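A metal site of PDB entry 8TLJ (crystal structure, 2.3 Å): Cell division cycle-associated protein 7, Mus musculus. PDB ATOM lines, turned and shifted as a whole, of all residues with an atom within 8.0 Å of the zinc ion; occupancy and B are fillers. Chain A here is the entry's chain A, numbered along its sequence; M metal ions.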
ATOM      1  N   HIS A  10     -16.279   3.006  21.789  1.00  0.00           N
ATOM      2  CA  HIS A  10     -15.510   1.867  22.279  1.00  0.00           C
ATOM      3  C   HIS A  10     -14.036   2.207  22.209  1.00  0.00           C
ATOM      4  O   HIS A  10     -13.491   2.433  21.124  1.00  0.00           O
ATOM      5  CB  HIS A  10     -15.821   0.606  21.479  1.00  0.00           C
ATOM      6  CG  HIS A  10     -14.958  -0.568  21.842  1.00  0.00           C
ATOM      7  ND1 HIS A  10     -14.003  -1.078  20.982  1.00  0.00           N
ATOM      8  CD2 HIS A  10     -14.900  -1.317  22.962  1.00  0.00           C
ATOM      9  CE1 HIS A  10     -13.404  -2.101  21.572  1.00  0.00           C
ATOM     10  NE2 HIS A  10     -13.931  -2.268  22.764  1.00  0.00           N
ATOM     11  N   ASN A  56     -12.778  -5.442  28.859  1.00  0.00           N
ATOM     12  CA  ASN A  56     -12.590  -4.525  27.736  1.00  0.00           C
ATOM     13  C   ASN A  56     -12.273  -5.357  26.502  1.00  0.00           C
ATOM     14  O   ASN A  56     -11.197  -5.969  26.423  1.00  0.00           O
ATOM     15  CB  ASN A  56     -11.469  -3.529  28.030  1.00  0.00           C
ATOM     16  CG  ASN A  56     -11.250  -2.557  26.889  1.00  0.00           C
ATOM     17  OD1 ASN A  56     -10.196  -2.571  26.233  1.00  0.00           O
ATOM     18  ND2 ASN A  56     -12.236  -1.701  26.635  1.00  0.00           N
ATOM     19  N   CYS A  57     -13.192  -5.405  25.552  1.00  0.00           N
ATOM     20  CA  CYS A  57     -12.972  -6.156  24.332  1.00  0.00           C
ATOM     21  C   CYS A  57     -11.911  -5.471  23.480  1.00  0.00           C
ATOM     22  O   CYS A  57     -11.976  -4.255  23.262  1.00  0.00           O
ATOM     23  CB  CYS A  57     -14.271  -6.313  23.547  1.00  0.00           C
ATOM     24  SG  CYS A  57     -14.088  -7.295  22.029  1.00  0.00           S
ATOM     25  N   ARG A  58     -10.946  -6.247  22.993  1.00  0.00           N
ATOM     26  CA  ARG A  58      -9.822  -5.697  22.237  1.00  0.00           C
ATOM     27  C   ARG A  58      -9.929  -6.002  20.742  1.00  0.00           C
ATOM     28  O   ARG A  58      -8.930  -5.887  20.020  1.00  0.00           O
ATOM     29  CB  ARG A  58      -8.506  -6.212  22.814  1.00  0.00           C
ATOM     30  CG  ARG A  58      -8.281  -5.750  24.236  1.00  0.00           C
ATOM     31  CD  ARG A  58      -6.898  -6.070  24.756  1.00  0.00           C
ATOM     32  NE  ARG A  58      -6.684  -5.448  26.058  1.00  0.00           N
ATOM     33  CZ  ARG A  58      -7.050  -5.969  27.210  1.00  0.00           C
ATOM     34  NH1 ARG A  58      -7.629  -7.168  27.272  1.00  0.00           N
ATOM     35  NH2 ARG A  58      -6.849  -5.289  28.339  1.00  0.00           N
ATOM     36  N   ASN A  59     -11.106  -6.394  20.270  1.00  0.00           N
ATOM     37  CA  ASN A  59     -11.340  -6.496  18.845  1.00  0.00           C
ATOM     38  C   ASN A  59     -11.558  -5.106  18.269  1.00  0.00           C
ATOM     39  O   ASN A  59     -12.453  -4.389  18.736  1.00  0.00           O
ATOM     40  CB  ASN A  59     -12.549  -7.391  18.569  1.00  0.00           C
ATOM     41  CG  ASN A  59     -12.832  -7.550  17.078  1.00  0.00           C
ATOM     42  OD1 ASN A  59     -11.974  -7.283  16.240  1.00  0.00           O
ATOM     43  ND2 ASN A  59     -14.036  -7.995  16.757  1.00  0.00           N
ATOM     44  N   PRO A  60     -10.760  -4.674  17.289  1.00  0.00           N
ATOM     45  CA  PRO A  60     -10.980  -3.344  16.710  1.00  0.00           C
ATOM     46  C   PRO A  60     -12.364  -3.158  16.099  1.00  0.00           C
ATOM     47  O   PRO A  60     -12.892  -2.046  16.125  1.00  0.00           O
ATOM     48  CB  PRO A  60      -9.878  -3.237  15.642  1.00  0.00           C
ATOM     49  CG  PRO A  60      -8.812  -4.167  16.129  1.00  0.00           C
ATOM     50  CD  PRO A  60      -9.530  -5.300  16.794  1.00  0.00           C
ATOM     51  N   ASP A  61     -12.958  -4.223  15.555  1.00  0.00           N
ATOM     52  CA  ASP A  61     -14.276  -4.122  14.949  1.00  0.00           C
ATOM     53  C   ASP A  61     -15.402  -4.125  15.967  1.00  0.00           C
ATOM     54  O   ASP A  61     -16.566  -3.973  15.583  1.00  0.00           O
ATOM     55  CB  ASP A  61     -14.476  -5.269  13.943  1.00  0.00           C
ATOM     56  CG  ASP A  61     -15.615  -4.990  12.973  1.00  0.00           C
ATOM     57  OD1 ASP A  61     -15.518  -4.013  12.197  1.00  0.00           O
ATOM     58  OD2 ASP A  61     -16.609  -5.747  12.982  1.00  0.00           O
ATOM     59  N   CYS A  62     -15.092  -4.301  17.253  1.00  0.00           N
ATOM     60  CA  CYS A  62     -16.106  -4.207  18.286  1.00  0.00           C
ATOM     61  C   CYS A  62     -16.578  -2.766  18.438  1.00  0.00           C
ATOM     62  O   CYS A  62     -15.923  -1.823  17.994  1.00  0.00           O
ATOM     63  CB  CYS A  62     -15.558  -4.737  19.617  1.00  0.00           C
ATOM     64  SG  CYS A  62     -16.814  -5.113  20.856  1.00  0.00           S
ATOM     65  N   TRP A  63     -17.736  -2.609  19.059  1.00  0.00           N
ATOM     66  CA  TRP A  63     -18.323  -1.292  19.230  1.00  0.00           C
ATOM     67  C   TRP A  63     -19.226  -1.293  20.452  1.00  0.00           C
ATOM     68  O   TRP A  63     -19.714  -2.350  20.888  1.00  0.00           O
ATOM     69  CB  TRP A  63     -19.127  -0.859  17.990  1.00  0.00           C
ATOM     70  CG  TRP A  63     -20.416  -1.595  17.838  1.00  0.00           C
ATOM     71  CD1 TRP A  63     -21.656  -1.150  18.180  1.00  0.00           C
ATOM     72  CD2 TRP A  63     -20.589  -2.922  17.326  1.00  0.00           C
ATOM     73  NE1 TRP A  63     -22.597  -2.114  17.911  1.00  0.00           N
ATOM     74  CE2 TRP A  63     -21.961  -3.212  17.390  1.00  0.00           C
ATOM     75  CE3 TRP A  63     -19.709  -3.887  16.824  1.00  0.00           C
ATOM     76  CZ2 TRP A  63     -22.493  -4.425  16.950  1.00  0.00           C
ATOM     77  CZ3 TRP A  63     -20.232  -5.092  16.396  1.00  0.00           C
ATOM     78  CH2 TRP A  63     -21.614  -5.352  16.467  1.00  0.00           C
ATOM     79  N   GLY A  64     -19.460  -0.107  20.998  1.00  0.00           N
ATOM     80  CA  GLY A  64     -20.383   0.063  22.093  1.00  0.00           C
ATOM     81  C   GLY A  64     -19.949  -0.664  23.356  1.00  0.00           C
ATOM     82  O   GLY A  64     -18.762  -0.806  23.651  1.00  0.00           O
ATOM     83  N   ILE A  65     -20.940  -1.125  24.116  1.00  0.00           N
ATOM     84  CA  ILE A  65     -20.714  -1.769  25.398  1.00  0.00           C
ATOM     85  C   ILE A  65     -20.898  -3.276  25.328  1.00  0.00           C
ATOM     86  O   ILE A  65     -20.884  -3.952  26.359  1.00  0.00           O
ATOM     87  CB  ILE A  65     -21.635  -1.177  26.483  1.00  0.00           C
ATOM     88  CG1 ILE A  65     -23.079  -1.575  26.203  1.00  0.00           C
ATOM     89  CG2 ILE A  65     -21.490   0.344  26.534  1.00  0.00           C
ATOM     90  CD1 ILE A  65     -23.980  -1.503  27.421  1.00  0.00           C
ATOM     91  N   ARG A  66     -21.083  -3.837  24.123  1.00  0.00           N
ATOM     92  CA  ARG A  66     -21.353  -5.269  24.004  1.00  0.00           C
ATOM     93  C   ARG A  66     -20.217  -6.114  24.563  1.00  0.00           C
ATOM     94  O   ARG A  66     -20.444  -7.271  24.916  1.00  0.00           O
ATOM     95  CB  ARG A  66     -21.593  -5.637  22.531  1.00  0.00           C
ATOM     96  CG  ARG A  66     -20.348  -5.536  21.662  1.00  0.00           C
ATOM     97  CD  ARG A  66     -20.701  -5.311  20.201  1.00  0.00           C
ATOM     98  NE  ARG A  66     -21.295  -6.481  19.573  1.00  0.00           N
ATOM     99  CZ  ARG A  66     -20.604  -7.454  18.990  1.00  0.00           C
ATOM    100  NH1 ARG A  66     -19.282  -7.440  18.976  1.00  0.00           N
ATOM    101  NH2 ARG A  66     -21.246  -8.463  18.426  1.00  0.00           N
ATOM    102  N   GLY A  67     -19.012  -5.568  24.661  1.00  0.00           N
ATOM    103  CA  GLY A  67     -17.860  -6.269  25.170  1.00  0.00           C
ATOM    104  C   GLY A  67     -17.598  -6.159  26.649  1.00  0.00           C
ATOM    105  O   GLY A  67     -16.589  -6.687  27.129  1.00  0.00           O
ATOM    106  N   GLN A  68     -18.474  -5.493  27.393  1.00  0.00           N
ATOM    107  CA  GLN A  68     -18.265  -5.235  28.810  1.00  0.00           C
ATOM    108  C   GLN A  68     -19.026  -6.277  29.627  1.00  0.00           C
ATOM    109  O   GLN A  68     -20.247  -6.363  29.537  1.00  0.00           O
ATOM    110  CB  GLN A  68     -18.726  -3.821  29.182  1.00  0.00           C
ATOM    111  CG  GLN A  68     -18.053  -2.733  28.351  1.00  0.00           C
ATOM    112  CD  GLN A  68     -18.582  -1.341  28.643  1.00  0.00           C
ATOM    113  OE1 GLN A  68     -19.456  -1.158  29.486  1.00  0.00           O
ATOM    114  NE2 GLN A  68     -18.047  -0.349  27.939  1.00  0.00           N
ATOM    115  N   PHE A  69     -18.287  -7.052  30.421  1.00  0.00           N
ATOM    116  CA  PHE A  69     -18.858  -8.117  31.230  1.00  0.00           C
ATOM    117  C   PHE A  69     -18.354  -8.023  32.665  1.00  0.00           C
ATOM    118  O   PHE A  69     -17.164  -7.774  32.901  1.00  0.00           O
ATOM    119  CB  PHE A  69     -18.519  -9.504  30.655  1.00  0.00           C
ATOM    120  CG  PHE A  69     -19.256  -9.836  29.395  1.00  0.00           C
ATOM    121  CD1 PHE A  69     -18.858  -9.311  28.173  1.00  0.00           C
ATOM    122  CD2 PHE A  69     -20.354 -10.679  29.431  1.00  0.00           C
ATOM    123  CE1 PHE A  69     -19.537  -9.615  27.014  1.00  0.00           C
ATOM    124  CE2 PHE A  69     -21.044 -10.982  28.271  1.00  0.00           C
ATOM    125  CZ  PHE A  69     -20.635 -10.450  27.062  1.00  0.00           C
ATOM    126  N   TRP A  91      -7.918 -10.721  23.843  1.00  0.00           N
ATOM    127  CA  TRP A  91      -9.229 -11.134  24.323  1.00  0.00           C
ATOM    128  C   TRP A  91     -10.342 -10.472  23.520  1.00  0.00           C
ATOM    129  O   TRP A  91     -10.359  -9.246  23.346  1.00  0.00           O
ATOM    130  CB  TRP A  91      -9.390 -10.799  25.803  1.00  0.00           C
ATOM    131  CG  TRP A  91     -10.649 -11.361  26.396  1.00  0.00           C
ATOM    132  CD1 TRP A  91     -10.835 -12.607  26.916  1.00  0.00           C
ATOM    133  CD2 TRP A  91     -11.904 -10.675  26.525  1.00  0.00           C
ATOM    134  NE1 TRP A  91     -12.126 -12.746  27.355  1.00  0.00           N
ATOM    135  CE2 TRP A  91     -12.804 -11.576  27.131  1.00  0.00           C
ATOM    136  CE3 TRP A  91     -12.354  -9.393  26.192  1.00  0.00           C
ATOM    137  CZ2 TRP A  91     -14.134 -11.237  27.406  1.00  0.00           C
ATOM    138  CZ3 TRP A  91     -13.665  -9.065  26.465  1.00  0.00           C
ATOM    139  CH2 TRP A  91     -14.545  -9.976  27.070  1.00  0.00           C
ATOM    140  N   HIS A  92     -11.282 -11.291  23.056  1.00  0.00           N
ATOM    141  CA  HIS A  92     -12.475 -10.834  22.359  1.00  0.00           C
ATOM    142  C   HIS A  92     -13.706 -11.184  23.194  1.00  0.00           C
ATOM    143  O   HIS A  92     -13.730 -12.220  23.859  1.00  0.00           O
ATOM    144  CB  HIS A  92     -12.596 -11.469  20.966  1.00  0.00           C
ATOM    145  CG  HIS A  92     -11.614 -10.924  19.968  1.00  0.00           C
ATOM    146  ND1 HIS A  92     -11.686 -11.223  18.629  1.00  0.00           N
ATOM    147  CD2 HIS A  92     -10.553 -10.101  20.119  1.00  0.00           C
ATOM    148  CE1 HIS A  92     -10.714 -10.612  17.983  1.00  0.00           C
ATOM    149  NE2 HIS A  92     -10.003  -9.922  18.870  1.00  0.00           N
ATOM    150  N   CYS A  93     -14.699 -10.304  23.161  1.00  0.00           N
ATOM    151  CA  CYS A  93     -15.914 -10.547  23.928  1.00  0.00           C
ATOM    152  C   CYS A  93     -16.718 -11.681  23.299  1.00  0.00           C
ATOM    153  O   CYS A  93     -16.566 -11.978  22.114  1.00  0.00           O
ATOM    154  CB  CYS A  93     -16.749  -9.276  24.007  1.00  0.00           C
ATOM    155  SG  CYS A  93     -17.500  -8.742  22.443  1.00  0.00           S
ATOM    156  N   PRO A  94     -17.566 -12.345  24.082  1.00  0.00           N
ATOM    157  CA  PRO A  94     -18.372 -13.448  23.542  1.00  0.00           C
ATOM    158  C   PRO A  94     -19.218 -13.014  22.352  1.00  0.00           C
ATOM    159  O   PRO A  94     -19.338 -13.782  21.380  1.00  0.00           O
ATOM    160  CB  PRO A  94     -19.247 -13.854  24.739  1.00  0.00           C
ATOM    161  CG  PRO A  94     -18.407 -13.518  25.922  1.00  0.00           C
ATOM    162  CD  PRO A  94     -17.635 -12.276  25.549  1.00  0.00           C
ATOM    163  N   PRO A  95     -19.823 -11.815  22.363  1.00  0.00           N
ATOM    164  CA  PRO A  95     -20.507 -11.366  21.132  1.00  0.00           C
ATOM    165  C   PRO A  95     -19.592 -11.304  19.913  1.00  0.00           C
ATOM    166  O   PRO A  95     -20.005 -11.668  18.812  1.00  0.00           O
ATOM    167  CB  PRO A  95     -21.048  -9.981  21.504  1.00  0.00           C
ATOM    168  CG  PRO A  95     -21.272 -10.070  22.960  1.00  0.00           C
ATOM    169  CD  PRO A  95     -20.134 -10.896  23.483  1.00  0.00           C
ATOM    170  N   CYS A  96     -18.352 -10.838  20.086  1.00  0.00           N
ATOM    171  CA  CYS A  96     -17.403 -10.852  18.975  1.00  0.00           C
ATOM    172  C   CYS A  96     -17.081 -12.280  18.544  1.00  0.00           C
ATOM    173  O   CYS A  96     -16.958 -12.564  17.350  1.00  0.00           O
ATOM    174  CB  CYS A  96     -16.132 -10.092  19.348  1.00  0.00           C
ATOM    175  SG  CYS A  96     -16.175  -8.310  18.976  1.00  0.00           S
ATOM    176  N   ARG A  97     -16.952 -13.190  19.508  1.00  0.00           N
ATOM    177  CA  ARG A  97     -16.744 -14.604  19.209  1.00  0.00           C
ATOM    178  C   ARG A  97     -18.021 -15.301  18.737  1.00  0.00           C
ATOM    179  O   ARG A  97     -17.951 -16.461  18.323  1.00  0.00           O
ATOM    180  CB  ARG A  97     -16.178 -15.324  20.427  1.00  0.00           C
ATOM    181  CG  ARG A  97     -14.697 -15.055  20.680  1.00  0.00           C
ATOM    182  CD  ARG A  97     -14.211 -15.717  21.970  1.00  0.00           C
ATOM    183  NE  ARG A  97     -14.488 -14.904  23.150  1.00  0.00           N
ATOM    184  CZ  ARG A  97     -14.273 -15.297  24.404  1.00  0.00           C
ATOM    185  NH1 ARG A  97     -13.789 -16.493  24.676  1.00  0.00           N
ATOM    186  NH2 ARG A  97     -14.543 -14.453  25.397  1.00  0.00           N
HETATM  187 ZN    ZN M   1     -16.191  -7.422  21.095  1.00  0.00          ZN
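The zinc ion is bound by SG of Cys 93, SG of Cys 96, SG of Cys 57 and SG of Cys 62.
SG of Cys 96 sits close to NH1 of Arg 66, 3.2 Å away.
ND2 of Asn 59 sits close to SG of Cys 96.
The backbone NH of Asn 59 lies close to the side-chain sulfur of Cys 57 (3.6 Å).
NE2 of His 10 is in hydrogen-bond range of O of Cys 57 (2.8 Å).
The backbone carbonyl oxygen (O) of Pro 95 lies close to the guanidinium group (NH2) of Arg 66, at 3.5 Å.
NH1 of Arg 66 touches the zinc ion, 3.7 Å away.
Of the 22 residues printed, 5 come within 4 Å of the zinc ion.
The nearest printed residue that does not touch the zinc ion is Asn 59 (4.4 Å).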
